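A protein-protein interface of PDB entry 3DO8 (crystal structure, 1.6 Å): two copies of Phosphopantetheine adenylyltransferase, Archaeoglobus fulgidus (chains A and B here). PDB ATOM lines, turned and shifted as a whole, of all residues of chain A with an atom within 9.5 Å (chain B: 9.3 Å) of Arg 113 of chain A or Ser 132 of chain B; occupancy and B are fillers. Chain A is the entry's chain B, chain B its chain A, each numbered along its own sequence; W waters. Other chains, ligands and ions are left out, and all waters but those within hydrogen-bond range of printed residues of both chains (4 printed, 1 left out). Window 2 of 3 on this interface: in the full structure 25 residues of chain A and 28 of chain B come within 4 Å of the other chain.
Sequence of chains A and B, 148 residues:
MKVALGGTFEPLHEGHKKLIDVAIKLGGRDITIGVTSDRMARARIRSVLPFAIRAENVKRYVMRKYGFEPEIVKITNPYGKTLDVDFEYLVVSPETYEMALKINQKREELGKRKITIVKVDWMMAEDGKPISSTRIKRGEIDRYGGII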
ATOM      1  N   THR A  82      10.725  25.480  -5.416  1.00  0.00           N
ATOM      2  CA  THR A  82      10.959  24.312  -4.579  1.00  0.00           C
ATOM      3  C   THR A  82      10.803  22.945  -5.267  1.00  0.00           C
ATOM      4  O   THR A  82      11.100  21.941  -4.648  1.00  0.00           O
ATOM      5  CB  THR A  82      10.065  24.314  -3.322  1.00  0.00           C
ATOM      6  OG1 THR A  82       8.699  24.134  -3.704  1.00  0.00           O
ATOM      7  CG2 THR A  82      10.237  25.628  -2.511  1.00  0.00           C
ATOM      8  N   LEU A  83      10.353  22.886  -6.521  1.00  0.00           N
ATOM      9  CA  LEU A  83      10.293  21.585  -7.224  1.00  0.00           C
ATOM     10  C   LEU A  83      11.522  21.350  -8.087  1.00  0.00           C
ATOM     11  O   LEU A  83      11.770  20.222  -8.527  1.00  0.00           O
ATOM     12  CB  LEU A  83       9.027  21.464  -8.080  1.00  0.00           C
ATOM     13  CG  LEU A  83       7.681  21.619  -7.366  1.00  0.00           C
ATOM     14  CD1 LEU A  83       6.554  21.526  -8.374  1.00  0.00           C
ATOM     15  CD2 LEU A  83       7.471  20.597  -6.258  1.00  0.00           C
ATOM     16  N   ASP A  84      12.283  22.415  -8.305  1.00  0.00           N
ATOM     17  CA  ASP A  84      13.379  22.445  -9.264  1.00  0.00           C
ATOM     18  C   ASP A  84      14.757  22.625  -8.631  1.00  0.00           C
ATOM     19  O   ASP A  84      15.771  22.369  -9.284  1.00  0.00           O
ATOM     20  CB  ASP A  84      13.155  23.620 -10.212  1.00  0.00           C
ATOM     21  CG  ASP A  84      13.938  23.498 -11.498  1.00  0.00           C
ATOM     22  OD1 ASP A  84      14.574  22.442 -11.741  1.00  0.00           O
ATOM     23  OD2 ASP A  84      13.901  24.476 -12.284  1.00  0.00           O
ATOM     24  N   VAL A  85      14.803  23.085  -7.385  1.00  0.00           N
ATOM     25  CA  VAL A  85      16.066  23.327  -6.705  1.00  0.00           C
ATOM     26  C   VAL A  85      16.120  22.385  -5.521  1.00  0.00           C
ATOM     27  O   VAL A  85      15.124  22.203  -4.806  1.00  0.00           O
ATOM     28  CB  VAL A  85      16.190  24.803  -6.269  1.00  0.00           C
ATOM     29  CG1 VAL A  85      17.376  25.012  -5.324  1.00  0.00           C
ATOM     30  CG2 VAL A  85      16.318  25.693  -7.514  1.00  0.00           C
ATOM     31  N   ASP A  86      17.279  21.773  -5.331  1.00  0.00           N
ATOM     32  CA  ASP A  86      17.463  20.849  -4.225  1.00  0.00           C
ATOM     33  C   ASP A  86      17.935  21.616  -2.991  1.00  0.00           C
ATOM     34  O   ASP A  86      19.092  21.511  -2.577  1.00  0.00           O
ATOM     35  CB  ASP A  86      18.448  19.748  -4.594  1.00  0.00           C
ATOM     36  CG  ASP A  86      17.902  18.815  -5.652  1.00  0.00           C
ATOM     37  OD1 ASP A  86      16.686  18.536  -5.662  1.00  0.00           O
ATOM     38  OD2 ASP A  86      18.697  18.346  -6.490  1.00  0.00           O
ATOM     39  N   PHE A  87      17.028  22.370  -2.396  1.00  0.00           N
ATOM     40  CA  PHE A  87      17.351  23.113  -1.184  1.00  0.00           C
ATOM     41  C   PHE A  87      17.737  22.187  -0.034  1.00  0.00           C
ATOM     42  O   PHE A  87      17.197  21.069   0.050  1.00  0.00           O
ATOM     43  CB  PHE A  87      16.119  23.891  -0.734  1.00  0.00           C
ATOM     44  CG  PHE A  87      15.756  25.027  -1.637  1.00  0.00           C
ATOM     45  CD1 PHE A  87      16.491  26.194  -1.615  1.00  0.00           C
ATOM     46  CD2 PHE A  87      14.670  24.932  -2.490  1.00  0.00           C
ATOM     47  CE1 PHE A  87      16.168  27.244  -2.441  1.00  0.00           C
ATOM     48  CE2 PHE A  87      14.333  25.998  -3.317  1.00  0.00           C
ATOM     49  CZ  PHE A  87      15.079  27.149  -3.289  1.00  0.00           C
ATOM     50  N   GLU A  88      18.630  22.664   0.855  1.00  0.00           N
ATOM     51  CA  GLU A  88      19.003  21.906   2.050  1.00  0.00           C
ATOM     52  C   GLU A  88      17.918  21.981   3.117  1.00  0.00           C
ATOM     53  O   GLU A  88      17.615  20.995   3.754  1.00  0.00           O
ATOM     54  CB  GLU A  88      20.296  22.434   2.690  1.00  0.00           C
ATOM     55  CG  GLU A  88      21.506  22.519   1.750  1.00  0.00           C
ATOM     56  CD  GLU A  88      22.801  22.951   2.439  1.00  0.00           C
ATOM     57  OE1 GLU A  88      22.769  23.640   3.493  1.00  0.00           O
ATOM     58  OE2 GLU A  88      23.876  22.577   1.907  1.00  0.00           O
ATOM     59  N   ILE A 103       4.674  20.533  -0.721  1.00  0.00           N
ATOM     60  CA  ILE A 103       5.851  20.645  -1.571  1.00  0.00           C
ATOM     61  C   ILE A 103       6.643  19.335  -1.552  1.00  0.00           C
ATOM     62  O   ILE A 103       6.961  18.795  -2.614  1.00  0.00           O
ATOM     63  CB  ILE A 103       6.747  21.836  -1.153  1.00  0.00           C
ATOM     64  CG1 ILE A 103       6.152  23.135  -1.669  1.00  0.00           C
ATOM     65  CG2 ILE A 103       8.185  21.680  -1.679  1.00  0.00           C
ATOM     66  CD1 ILE A 103       6.725  24.395  -0.921  1.00  0.00           C
ATOM     67  N   ASN A 104       6.922  18.798  -0.367  1.00  0.00           N
ATOM     68  CA  ASN A 104       7.651  17.540  -0.265  1.00  0.00           C
ATOM     69  C   ASN A 104       6.891  16.362  -0.858  1.00  0.00           C
ATOM     70  O   ASN A 104       7.487  15.506  -1.501  1.00  0.00           O
ATOM     71  CB  ASN A 104       8.062  17.221   1.166  1.00  0.00           C
ATOM     72  CG  ASN A 104       9.443  17.785   1.537  1.00  0.00           C
ATOM     73  OD1 ASN A 104       9.804  17.822   2.721  1.00  0.00           O
ATOM     74  ND2 ASN A 104      10.200  18.222   0.544  1.00  0.00           N
ATOM     75  N   GLN A 105       5.580  16.314  -0.628  1.00  0.00           N
ATOM     76  CA  GLN A 105       4.768  15.247  -1.249  1.00  0.00           C
ATOM     77  C   GLN A 105       4.913  15.303  -2.774  1.00  0.00           C
ATOM     78  O   GLN A 105       5.121  14.277  -3.408  1.00  0.00           O
ATOM     79  CB  GLN A 105       3.297  15.348  -0.822  1.00  0.00           C
ATOM     80  CG  GLN A 105       2.411  14.256  -1.373  1.00  0.00           C
ATOM     81  CD  GLN A 105       0.933  14.573  -1.158  1.00  0.00           C
ATOM     82  OE1 GLN A 105       0.585  15.420  -0.326  1.00  0.00           O
ATOM     83  NE2 GLN A 105       0.065  13.915  -1.921  1.00  0.00           N
ATOM     84  N   LYS A 106       4.857  16.497  -3.346  1.00  0.00           N
ATOM     85  CA  LYS A 106       5.003  16.673  -4.785  1.00  0.00           C
ATOM     86  C   LYS A 106       6.401  16.327  -5.269  1.00  0.00           C
ATOM     87  O   LYS A 106       6.547  15.642  -6.251  1.00  0.00           O
ATOM     88  CB  LYS A 106       4.652  18.095  -5.210  1.00  0.00           C
ATOM     89  CG  LYS A 106       4.585  18.306  -6.702  1.00  0.00           C
ATOM     90  CD  LYS A 106       3.374  17.567  -7.298  1.00  0.00           C
ATOM     91  CE  LYS A 106       3.268  17.755  -8.791  1.00  0.00           C
ATOM     92  NZ  LYS A 106       2.277  16.801  -9.377  1.00  0.00           N
ATOM     93  N   ARG A 107       7.433  16.787  -4.569  1.00  0.00           N
ATOM     94  CA  ARG A 107       8.812  16.377  -4.889  1.00  0.00           C
ATOM     95  C   ARG A 107       8.961  14.857  -4.942  1.00  0.00           C
ATOM     96  O   ARG A 107       9.539  14.323  -5.880  1.00  0.00           O
ATOM     97  CB  ARG A 107       9.810  16.978  -3.864  1.00  0.00           C
ATOM     98  CG  ARG A 107       9.970  18.463  -4.050  1.00  0.00           C
ATOM     99  CD  ARG A 107      10.996  19.096  -3.085  1.00  0.00           C
ATOM    100  NE  ARG A 107      12.316  18.490  -3.255  1.00  0.00           N
ATOM    101  CZ  ARG A 107      13.285  18.954  -4.038  1.00  0.00           C
ATOM    102  NH1 ARG A 107      13.129  20.070  -4.748  1.00  0.00           N
ATOM    103  NH2 ARG A 107      14.435  18.297  -4.107  1.00  0.00           N
ATOM    104  N   GLU A 108       8.430  14.156  -3.950  1.00  0.00           N
ATOM    105  CA  GLU A 108       8.591  12.718  -3.893  1.00  0.00           C
ATOM    106  C   GLU A 108       7.850  12.072  -5.056  1.00  0.00           C
ATOM    107  O   GLU A 108       8.366  11.139  -5.637  1.00  0.00           O
ATOM    108  CB  GLU A 108       8.102  12.153  -2.562  1.00  0.00           C
ATOM    109  CG  GLU A 108       8.314  10.672  -2.446  1.00  0.00           C
ATOM    110  CD  GLU A 108       8.061  10.162  -1.059  1.00  0.00           C
ATOM    111  OE1 GLU A 108       7.011  10.540  -0.485  1.00  0.00           O
ATOM    112  OE2 GLU A 108       8.909   9.374  -0.542  1.00  0.00           O
ATOM    113  N   GLU A 109       6.688  12.612  -5.392  1.00  0.00           N
ATOM    114  CA  GLU A 109       5.901  12.092  -6.523  1.00  0.00           C
ATOM    115  C   GLU A 109       6.668  12.249  -7.840  1.00  0.00           C
ATOM    116  O   GLU A 109       6.511  11.435  -8.753  1.00  0.00           O
ATOM    117  CB  GLU A 109       4.537  12.767  -6.584  1.00  0.00           C
ATOM    118  CG  GLU A 109       3.597  12.243  -5.479  1.00  0.00           C
ATOM    119  CD  GLU A 109       2.339  13.062  -5.265  1.00  0.00           C
ATOM    120  OE1 GLU A 109       2.058  14.004  -6.057  1.00  0.00           O
ATOM    121  OE2 GLU A 109       1.617  12.739  -4.287  1.00  0.00           O
ATOM    122  N   LEU A 110       7.518  13.275  -7.917  1.00  0.00           N
ATOM    123  CA  LEU A 110       8.391  13.524  -9.070  1.00  0.00           C
ATOM    124  C   LEU A 110       9.809  12.915  -8.969  1.00  0.00           C
ATOM    125  O   LEU A 110      10.676  13.180  -9.805  1.00  0.00           O
ATOM    126  CB  LEU A 110       8.473  15.026  -9.351  1.00  0.00           C
ATOM    127  CG  LEU A 110       7.133  15.772  -9.484  1.00  0.00           C
ATOM    128  CD1 LEU A 110       7.382  17.265  -9.534  1.00  0.00           C
ATOM    129  CD2 LEU A 110       6.300  15.283 -10.686  1.00  0.00           C
ATOM    130  N   GLY A 111      10.046  12.078  -7.969  1.00  0.00           N
ATOM    131  CA  GLY A 111      11.298  11.337  -7.856  1.00  0.00           C
ATOM    132  C   GLY A 111      12.418  12.185  -7.293  1.00  0.00           C
ATOM    133  O   GLY A 111      13.568  11.755  -7.264  1.00  0.00           O
ATOM    134  N   LYS A 112      12.056  13.362  -6.768  1.00  0.00           N
ATOM    135  CA  LYS A 112      13.033  14.292  -6.167  1.00  0.00           C
ATOM    136  C   LYS A 112      13.197  13.984  -4.678  1.00  0.00           C
ATOM    137  O   LYS A 112      12.282  13.513  -4.043  1.00  0.00           O
ATOM    138  CB  LYS A 112      12.555  15.729  -6.296  1.00  0.00           C
ATOM    139  CG  LYS A 112      12.336  16.242  -7.698  1.00  0.00           C
ATOM    140  CD  LYS A 112      13.611  16.295  -8.439  1.00  0.00           C
ATOM    141  CE  LYS A 112      13.608  17.407  -9.504  1.00  0.00           C
ATOM    142  NZ  LYS A 112      14.991  17.713  -9.995  1.00  0.00           N
ATOM    143  N   ARG A 113      14.374  14.240  -4.128  1.00  0.00           N
ATOM    144  CA  ARG A 113      14.581  14.065  -2.691  1.00  0.00           C
ATOM    145  C   ARG A 113      13.778  15.117  -1.962  1.00  0.00           C
ATOM    146  O   ARG A 113      13.713  16.234  -2.393  1.00  0.00           O
ATOM    147  CB  ARG A 113      16.050  14.254  -2.350  1.00  0.00           C
ATOM    148  CG  ARG A 113      16.986  13.183  -2.907  1.00  0.00           C
ATOM    149  CD  ARG A 113      18.452  13.659  -2.892  1.00  0.00           C
ATOM    150  NE  ARG A 113      18.685  14.652  -3.949  1.00  0.00           N
ATOM    151  CZ  ARG A 113      19.638  15.587  -3.954  1.00  0.00           C
ATOM    152  NH1 ARG A 113      20.517  15.726  -2.946  1.00  0.00           N
ATOM    153  NH2 ARG A 113      19.704  16.407  -4.992  1.00  0.00           N
ATOM    154  N   LYS A 114      13.174  14.740  -0.850  1.00  0.00           N
ATOM    155  CA  LYS A 114      12.471  15.719  -0.002  1.00  0.00           C
ATOM    156  C   LYS A 114      13.485  16.673   0.658  1.00  0.00           C
ATOM    157  O   LYS A 114      14.625  16.277   0.915  1.00  0.00           O
ATOM    158  CB  LYS A 114      11.659  14.991   1.043  1.00  0.00           C
ATOM    159  CG  LYS A 114      10.461  14.266   0.444  1.00  0.00           C
ATOM    160  CD  LYS A 114       9.706  13.517   1.536  1.00  0.00           C
ATOM    161  CE  LYS A 114       8.477  12.890   0.990  1.00  0.00           C
ATOM    162  NZ  LYS A 114       7.729  12.088   2.005  1.00  0.00           N
ATOM    163  N   ILE A 115      13.048  17.901   0.906  1.00  0.00           N
ATOM    164  CA  ILE A 115      13.838  18.921   1.594  1.00  0.00           C
ATOM    165  C   ILE A 115      13.547  18.816   3.073  1.00  0.00           C
ATOM    166  O   ILE A 115      12.414  18.613   3.469  1.00  0.00           O
ATOM    167  CB  ILE A 115      13.503  20.347   1.096  1.00  0.00           C
ATOM    168  CG1 ILE A 115      13.600  20.439  -0.452  1.00  0.00           C
ATOM    169  CG2 ILE A 115      14.405  21.379   1.799  1.00  0.00           C
ATOM    170  CD1 ILE A 115      12.918  21.638  -1.073  1.00  0.00           C
ATOM    171  N   THR A 116      14.552  18.968   3.920  1.00  0.00           N
ATOM    172  CA  THR A 116      14.274  18.981   5.359  1.00  0.00           C
ATOM    173  C   THR A 116      13.518  20.251   5.715  1.00  0.00           C
ATOM    174  O   THR A 116      14.001  21.358   5.473  1.00  0.00           O
ATOM    175  CB  THR A 116      15.579  18.921   6.165  1.00  0.00           C
ATOM    176  OG1 THR A 116      16.324  17.733   5.820  1.00  0.00           O
ATOM    177  CG2 THR A 116      15.318  18.934   7.674  1.00  0.00           C
ATOM    178  N   ILE A 117      12.333  20.088   6.272  1.00  0.00           N
ATOM    179  CA  ILE A 117      11.503  21.211   6.727  1.00  0.00           C
ATOM    180  C   ILE A 117      11.869  21.605   8.158  1.00  0.00           C
ATOM    181  O   ILE A 117      12.033  20.743   9.032  1.00  0.00           O
ATOM    182  CB  ILE A 117      10.018  20.877   6.651  1.00  0.00           C
ATOM    183  CG1 ILE A 117       9.613  20.576   5.206  1.00  0.00           C
ATOM    184  CG2 ILE A 117       9.149  21.990   7.300  1.00  0.00           C
ATOM    185  CD1 ILE A 117       8.228  19.965   5.113  1.00  0.00           C
ATOM    186  N   GLU B  14      20.978   9.710  10.827  1.00  0.00           N
ATOM    187  CA  GLU B  14      20.966  10.875   9.954  1.00  0.00           C
ATOM    188  C   GLU B  14      19.997  11.942  10.474  1.00  0.00           C
ATOM    189  O   GLU B  14      20.263  13.140  10.366  1.00  0.00           O
ATOM    190  CB  GLU B  14      20.637  10.472   8.503  1.00  0.00           C
ATOM    191  CG  GLU B  14      20.480  11.675   7.559  1.00  0.00           C
ATOM    192  CD  GLU B  14      21.683  12.636   7.588  1.00  0.00           C
ATOM    193  OE1 GLU B  14      22.846  12.143   7.681  1.00  0.00           O
ATOM    194  OE2 GLU B  14      21.482  13.881   7.498  1.00  0.00           O
ATOM    195  N   LYS B  18      20.826  15.867  11.419  1.00  0.00           N
ATOM    196  CA  LYS B  18      20.114  17.064  10.972  1.00  0.00           C
ATOM    197  C   LYS B  18      19.818  17.981  12.148  1.00  0.00           C
ATOM    198  O   LYS B  18      19.986  19.201  12.058  1.00  0.00           O
ATOM    199  CB  LYS B  18      18.839  16.711  10.237  1.00  0.00           C
ATOM    200  CG  LYS B  18      19.065  16.002   8.910  1.00  0.00           C
ATOM    201  CD  LYS B  18      17.776  15.488   8.280  1.00  0.00           C
ATOM    202  CE  LYS B  18      18.011  15.099   6.811  1.00  0.00           C
ATOM    203  NZ  LYS B  18      16.728  14.643   6.222  1.00  0.00           N
ATOM    204  N   ASP B 121      11.791  18.446  10.740  1.00  0.00           N
ATOM    205  CA  ASP B 121      11.138  17.218  10.233  1.00  0.00           C
ATOM    206  C   ASP B 121      12.230  16.350   9.625  1.00  0.00           C
ATOM    207  O   ASP B 121      12.600  16.459   8.462  1.00  0.00           O
ATOM    208  CB  ASP B 121      10.046  17.550   9.228  1.00  0.00           C
ATOM    209  CG  ASP B 121       8.698  17.912   9.878  1.00  0.00           C
ATOM    210  OD1 ASP B 121       8.566  18.017  11.119  1.00  0.00           O
ATOM    211  OD2 ASP B 121       7.739  18.063   9.106  1.00  0.00           O
ATOM    212  N   TRP B 122      12.768  15.502  10.462  1.00  0.00           N
ATOM    213  CA  TRP B 122      14.009  14.811  10.155  1.00  0.00           C
ATOM    214  C   TRP B 122      13.865  13.570   9.282  1.00  0.00           C
ATOM    215  O   TRP B 122      14.879  12.907   9.014  1.00  0.00           O
ATOM    216  CB  TRP B 122      14.732  14.491  11.477  1.00  0.00           C
ATOM    217  CG  TRP B 122      14.077  13.449  12.341  1.00  0.00           C
ATOM    218  CD1 TRP B 122      12.879  12.808  12.126  1.00  0.00           C
ATOM    219  CD2 TRP B 122      14.577  12.947  13.581  1.00  0.00           C
ATOM    220  NE1 TRP B 122      12.619  11.925  13.155  1.00  0.00           N
ATOM    221  CE2 TRP B 122      13.656  11.977  14.048  1.00  0.00           C
ATOM    222  CE3 TRP B 122      15.711  13.217  14.341  1.00  0.00           C
ATOM    223  CZ2 TRP B 122      13.840  11.288  15.240  1.00  0.00           C
ATOM    224  CZ3 TRP B 122      15.903  12.517  15.513  1.00  0.00           C
ATOM    225  CH2 TRP B 122      14.974  11.571  15.957  1.00  0.00           C
ATOM    226  N   MET B 123      12.627  13.250   8.898  1.00  0.00           N
ATOM    227  CA  MET B 123      12.312  12.173   7.926  1.00  0.00           C
ATOM    228  C   MET B 123      13.002  10.839   8.194  1.00  0.00           C
ATOM    229  O   MET B 123      13.712  10.272   7.334  1.00  0.00           O
ATOM    230  CB  MET B 123      12.592  12.678   6.523  1.00  0.00           C
ATOM    231  CG  MET B 123      11.677  13.854   6.164  1.00  0.00           C
ATOM    232  SD  MET B 123      12.032  14.597   4.580  1.00  0.00           S
ATOM    233  CE  MET B 123      13.741  15.059   4.718  1.00  0.00           C
ATOM    234  N   MET B 124      12.753  10.336   9.394  1.00  0.00           N
ATOM    235  CA  MET B 124      13.174   8.994   9.780  1.00  0.00           C
ATOM    236  C   MET B 124      11.979   8.043   9.762  1.00  0.00           C
ATOM    237  O   MET B 124      10.839   8.488   9.604  1.00  0.00           O
ATOM    238  CB  MET B 124      13.793   9.038  11.176  1.00  0.00           C
ATOM    239  CG  MET B 124      15.135   9.755  11.228  1.00  0.00           C
ATOM    240  SD  MET B 124      16.436   8.989  10.224  1.00  0.00           S
ATOM    241  CE  MET B 124      16.611   7.415  11.061  1.00  0.00           C
ATOM    242  N   SER B 132      14.542   9.339   1.644  1.00  0.00           N
ATOM    243  CA  SER B 132      15.340  10.350   0.949  1.00  0.00           C
ATOM    244  C   SER B 132      15.512  11.584   1.791  1.00  0.00           C
ATOM    245  O   SER B 132      14.724  11.842   2.725  1.00  0.00           O
ATOM    246  CB  SER B 132      14.619  10.871  -0.296  1.00  0.00           C
ATOM    247  OG  SER B 132      13.891  12.073   0.052  1.00  0.00           O
ATOM    248  N   SER B 133      16.519  12.368   1.423  1.00  0.00           N
ATOM    249  CA  SER B 133      16.469  13.819   1.626  1.00  0.00           C
ATOM    250  C   SER B 133      17.619  14.475   0.875  1.00  0.00           C
ATOM    251  O   SER B 133      18.659  13.838   0.623  1.00  0.00           O
ATOM    252  CB  SER B 133      16.483  14.212   3.108  1.00  0.00           C
ATOM    253  OG  SER B 133      17.581  13.639   3.789  1.00  0.00           O
ATOM    254  N   THR B 134      17.399  15.725   0.473  1.00  0.00           N
ATOM    255  CA  THR B 134      18.409  16.516  -0.218  1.00  0.00           C
ATOM    256  C   THR B 134      19.646  16.589   0.680  1.00  0.00           C
ATOM    257  O   THR B 134      19.537  16.554   1.920  1.00  0.00           O
ATOM    258  CB  THR B 134      17.928  17.962  -0.495  1.00  0.00           C
ATOM    259  OG1 THR B 134      17.410  18.512   0.716  1.00  0.00           O
ATOM    260  CG2 THR B 134      16.847  18.015  -1.563  1.00  0.00           C
ATOM    261  N   ARG B 135      20.810  16.708   0.045  1.00  0.00           N
ATOM    262  CA  ARG B 135      22.064  16.777   0.769  1.00  0.00           C
ATOM    263  C   ARG B 135      22.100  18.085   1.548  1.00  0.00           C
ATOM    264  O   ARG B 135      21.593  19.118   1.075  1.00  0.00           O
ATOM    265  CB  ARG B 135      23.256  16.699  -0.185  1.00  0.00           C
ATOM    266  CG  ARG B 135      24.603  16.693   0.538  1.00  0.00           C
ATOM    267  CD  ARG B 135      25.748  16.196  -0.363  1.00  0.00           C
ATOM    268  NE  ARG B 135      26.904  15.738   0.424  1.00  0.00           N
ATOM    269  CZ  ARG B 135      27.101  14.495   0.879  1.00  0.00           C
ATOM    270  NH1 ARG B 135      26.231  13.514   0.632  1.00  0.00           N
ATOM    271  NH2 ARG B 135      28.198  14.226   1.589  1.00  0.00           N
ATOM    272  N   ILE B 136      22.644  18.014   2.764  1.00  0.00           N
ATOM    273  CA  ILE B 136      22.922  19.198   3.559  1.00  0.00           C
ATOM    274  C   ILE B 136      24.425  19.259   3.815  1.00  0.00           C
ATOM    275  O   ILE B 136      25.021  18.296   4.317  1.00  0.00           O
ATOM    276  CB  ILE B 136      22.214  19.178   4.920  1.00  0.00           C
ATOM    277  CG1 ILE B 136      20.688  19.202   4.756  1.00  0.00           C
ATOM    278  CG2 ILE B 136      22.671  20.366   5.748  1.00  0.00           C
ATOM    279  CD1 ILE B 136      19.943  18.557   5.915  1.00  0.00           C
ATOM    280  N   LYS B 137      25.033  20.387   3.469  1.00  0.00           N
ATOM    281  CA  LYS B 137      26.438  20.606   3.756  1.00  0.00           C
ATOM    282  C   LYS B 137      26.605  20.946   5.244  1.00  0.00           C
ATOM    283  O   LYS B 137      26.237  22.043   5.686  1.00  0.00           O
ATOM    284  CB  LYS B 137      26.984  21.715   2.861  1.00  0.00           C
ATOM    285  CG  LYS B 137      26.909  21.357   1.369  1.00  0.00           C
ATOM    286  CD  LYS B 137      28.151  20.624   0.875  1.00  0.00           C
ATOM    287  CE  LYS B 137      29.316  21.585   0.663  1.00  0.00           C
ATOM    288  NZ  LYS B 137      30.352  21.032  -0.263  1.00  0.00           N
HETATM  289  O   HOH W   1      11.652  10.848  -0.732  1.00  0.00           O
HETATM  290  O   HOH W   2      20.920  19.893  -1.206  1.00  0.00           O
HETATM  291  O   HOH W   3       8.456  13.441   4.636  1.00  0.00           O
HETATM  292  O   HOH W   4      17.448  18.377   3.440  1.00  0.00           O
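No position is printed for both chains.
Hydrophobic or aromatic side chains of chain B that line the printed part of chain A: Met 123 and Ile 136. Of the 22 printed residues of chain A, 9 touch a printed residue of chain B. Printed residues of chain A that touch a printed residue of chain B: Asp 86, Phe 87, Glu 88, Arg 107, Arg 113, Lys 114, Ile 115, Thr 116 and Ile 117. Among the printed residues, no Asp or Glu carboxylate lies within 4 Å of a Lys or Arg side-chain nitrogen of the other chain.
N of Asp 121 of chain B lies within hydrogen-bond range of O of Ile 117 of chain A. The backbone NH (N) of Thr 134 of chain B lies within hydrogen-bond range of the backbone carbonyl oxygen (O) of Lys 114 of chain A (2.9 Å). The side-chain hydroxyl (OG1) of Thr 134 of chain B sits at hydrogen-bond distance from the backbone carbonyl oxygen (O) of Phe 87 of chain A. The guanidinium group (NH1) of Arg 113 of chain A lies close to the backbone NH (N) of Arg 135 of chain B (3.2 Å). The side-chain amino group (NZ) of Lys 18 of chain B lies within hydrogen-bond range of the side-chain hydroxyl (OG1) of Thr 116 of chain A (3.1 Å). OE2 of Glu 88 of chain A sits at hydrogen-bond distance from N of Lys 137 of chain B. OG of Ser 132 of chain B sits at hydrogen-bond distance from N of Lys 114 of chain A.
Water W2 lies within hydrogen-bond range of O of Arg 135 of chain B (2.5 Å) and O of Asp 86 of chain A (2.8 Å). Water W4 lies within hydrogen-bond range of the backbone carbonyl oxygen (O) of Glu 88 of chain A (2.6 Å), the side-chain hydroxyl (OG1) of Thr 116 of chain A (2.7 Å) and the side-chain hydroxyl (OG1) of Thr 134 of chain B (2.7 Å). Water W1 bridges OG of Ser 132 of chain B (2.7 Å) and OE2 of Glu 108 of chain A (3.1 Å). Water W3 bridges the side-chain amino group of Lys 114 of chain A (3.0 Å) and the side-chain sulfur of Met 123 of chain B (3.8 Å).
Leu 83 of chain A touches none of the printed residues of chain B. Of the printed residues of chain B, Phe 87 of chain A touches Thr 134. Of chain B, only Ser 132, Ser 133, Thr 134 and Arg 135 come within 4 Å of Arg 113 of chain A. Of the printed residues of chain A, Asp 121 of chain B touches Thr 116 and Ile 117. Of the printed residues of chain A, Met 123 of chain B touches Lys 114 (3.6 Å), Ile 115 (3.99 Å) and Thr 116 (3.9 Å). Ser 132 of chain B touches just these residues of chain A: Arg 113 and Lys 114. Of chain A, only Arg 113 and Lys 114 come within 4 Å of Ser 133 of chain B. Thr 134 of chain B touches just these residues of chain A: Asp 86, Phe 87, Glu 88, Arg 107, Arg 113, Lys 114 and Ile 115. The nearest residue of chain B that does not touch Arg 113 of chain A is Ile 136 of chain B (6.5 Å).
CG2 of Thr 134 of chain B touches CB of Asp 86 of chain A, at 3.8 Å. O of Glu 88 of chain A touches OG1 of Thr 134 of chain B, at 3.9 Å. Arg 135 of chain B touches Glu 88 of chain A (O to CG, 3.5 Å). Ile 136 of chain B touches Glu 88 of chain A (CG1 to O, 3.7 Å). Ser 132 of chain B touches Arg 113 of chain A. Lys 114 of chain A touches Met 123 of chain B (CB to SD, 3.6 Å). Ser 133 of chain B touches Lys 114 of chain A. Ile 115 of chain A touches Met 123 of chain B (O to CE, 3.99 Å). Ile 115 of chain A touches Thr 134 of chain B. OG1 of Thr 116 of chain A touches CD1 of Ile 136 of chain B, 3.7 Å away.
OD2 of Asp 86 of chain A is in salt-bridge range of NH2 of Arg 113 of chain A, 2.6 Å away. The backbone carbonyl oxygen of Arg 113 of chain A sits at hydrogen-bond distance from the guanidinium group of Arg 107 of chain A (2.8 Å). The backbone carbonyl oxygen of Arg 107 of chain A is in hydrogen-bond range of the backbone NH of Lys 112 of chain A (2.8 Å). The side-chain amino group (NZ) of Lys 18 of chain B sits at hydrogen-bond distance from the side-chain hydroxyl (OG) of Ser 133 of chain B. The guanidinium group of Arg 107 of chain A is in hydrogen-bond range of the backbone carbonyl oxygen of Val 85 of chain A, 2.9 Å away.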
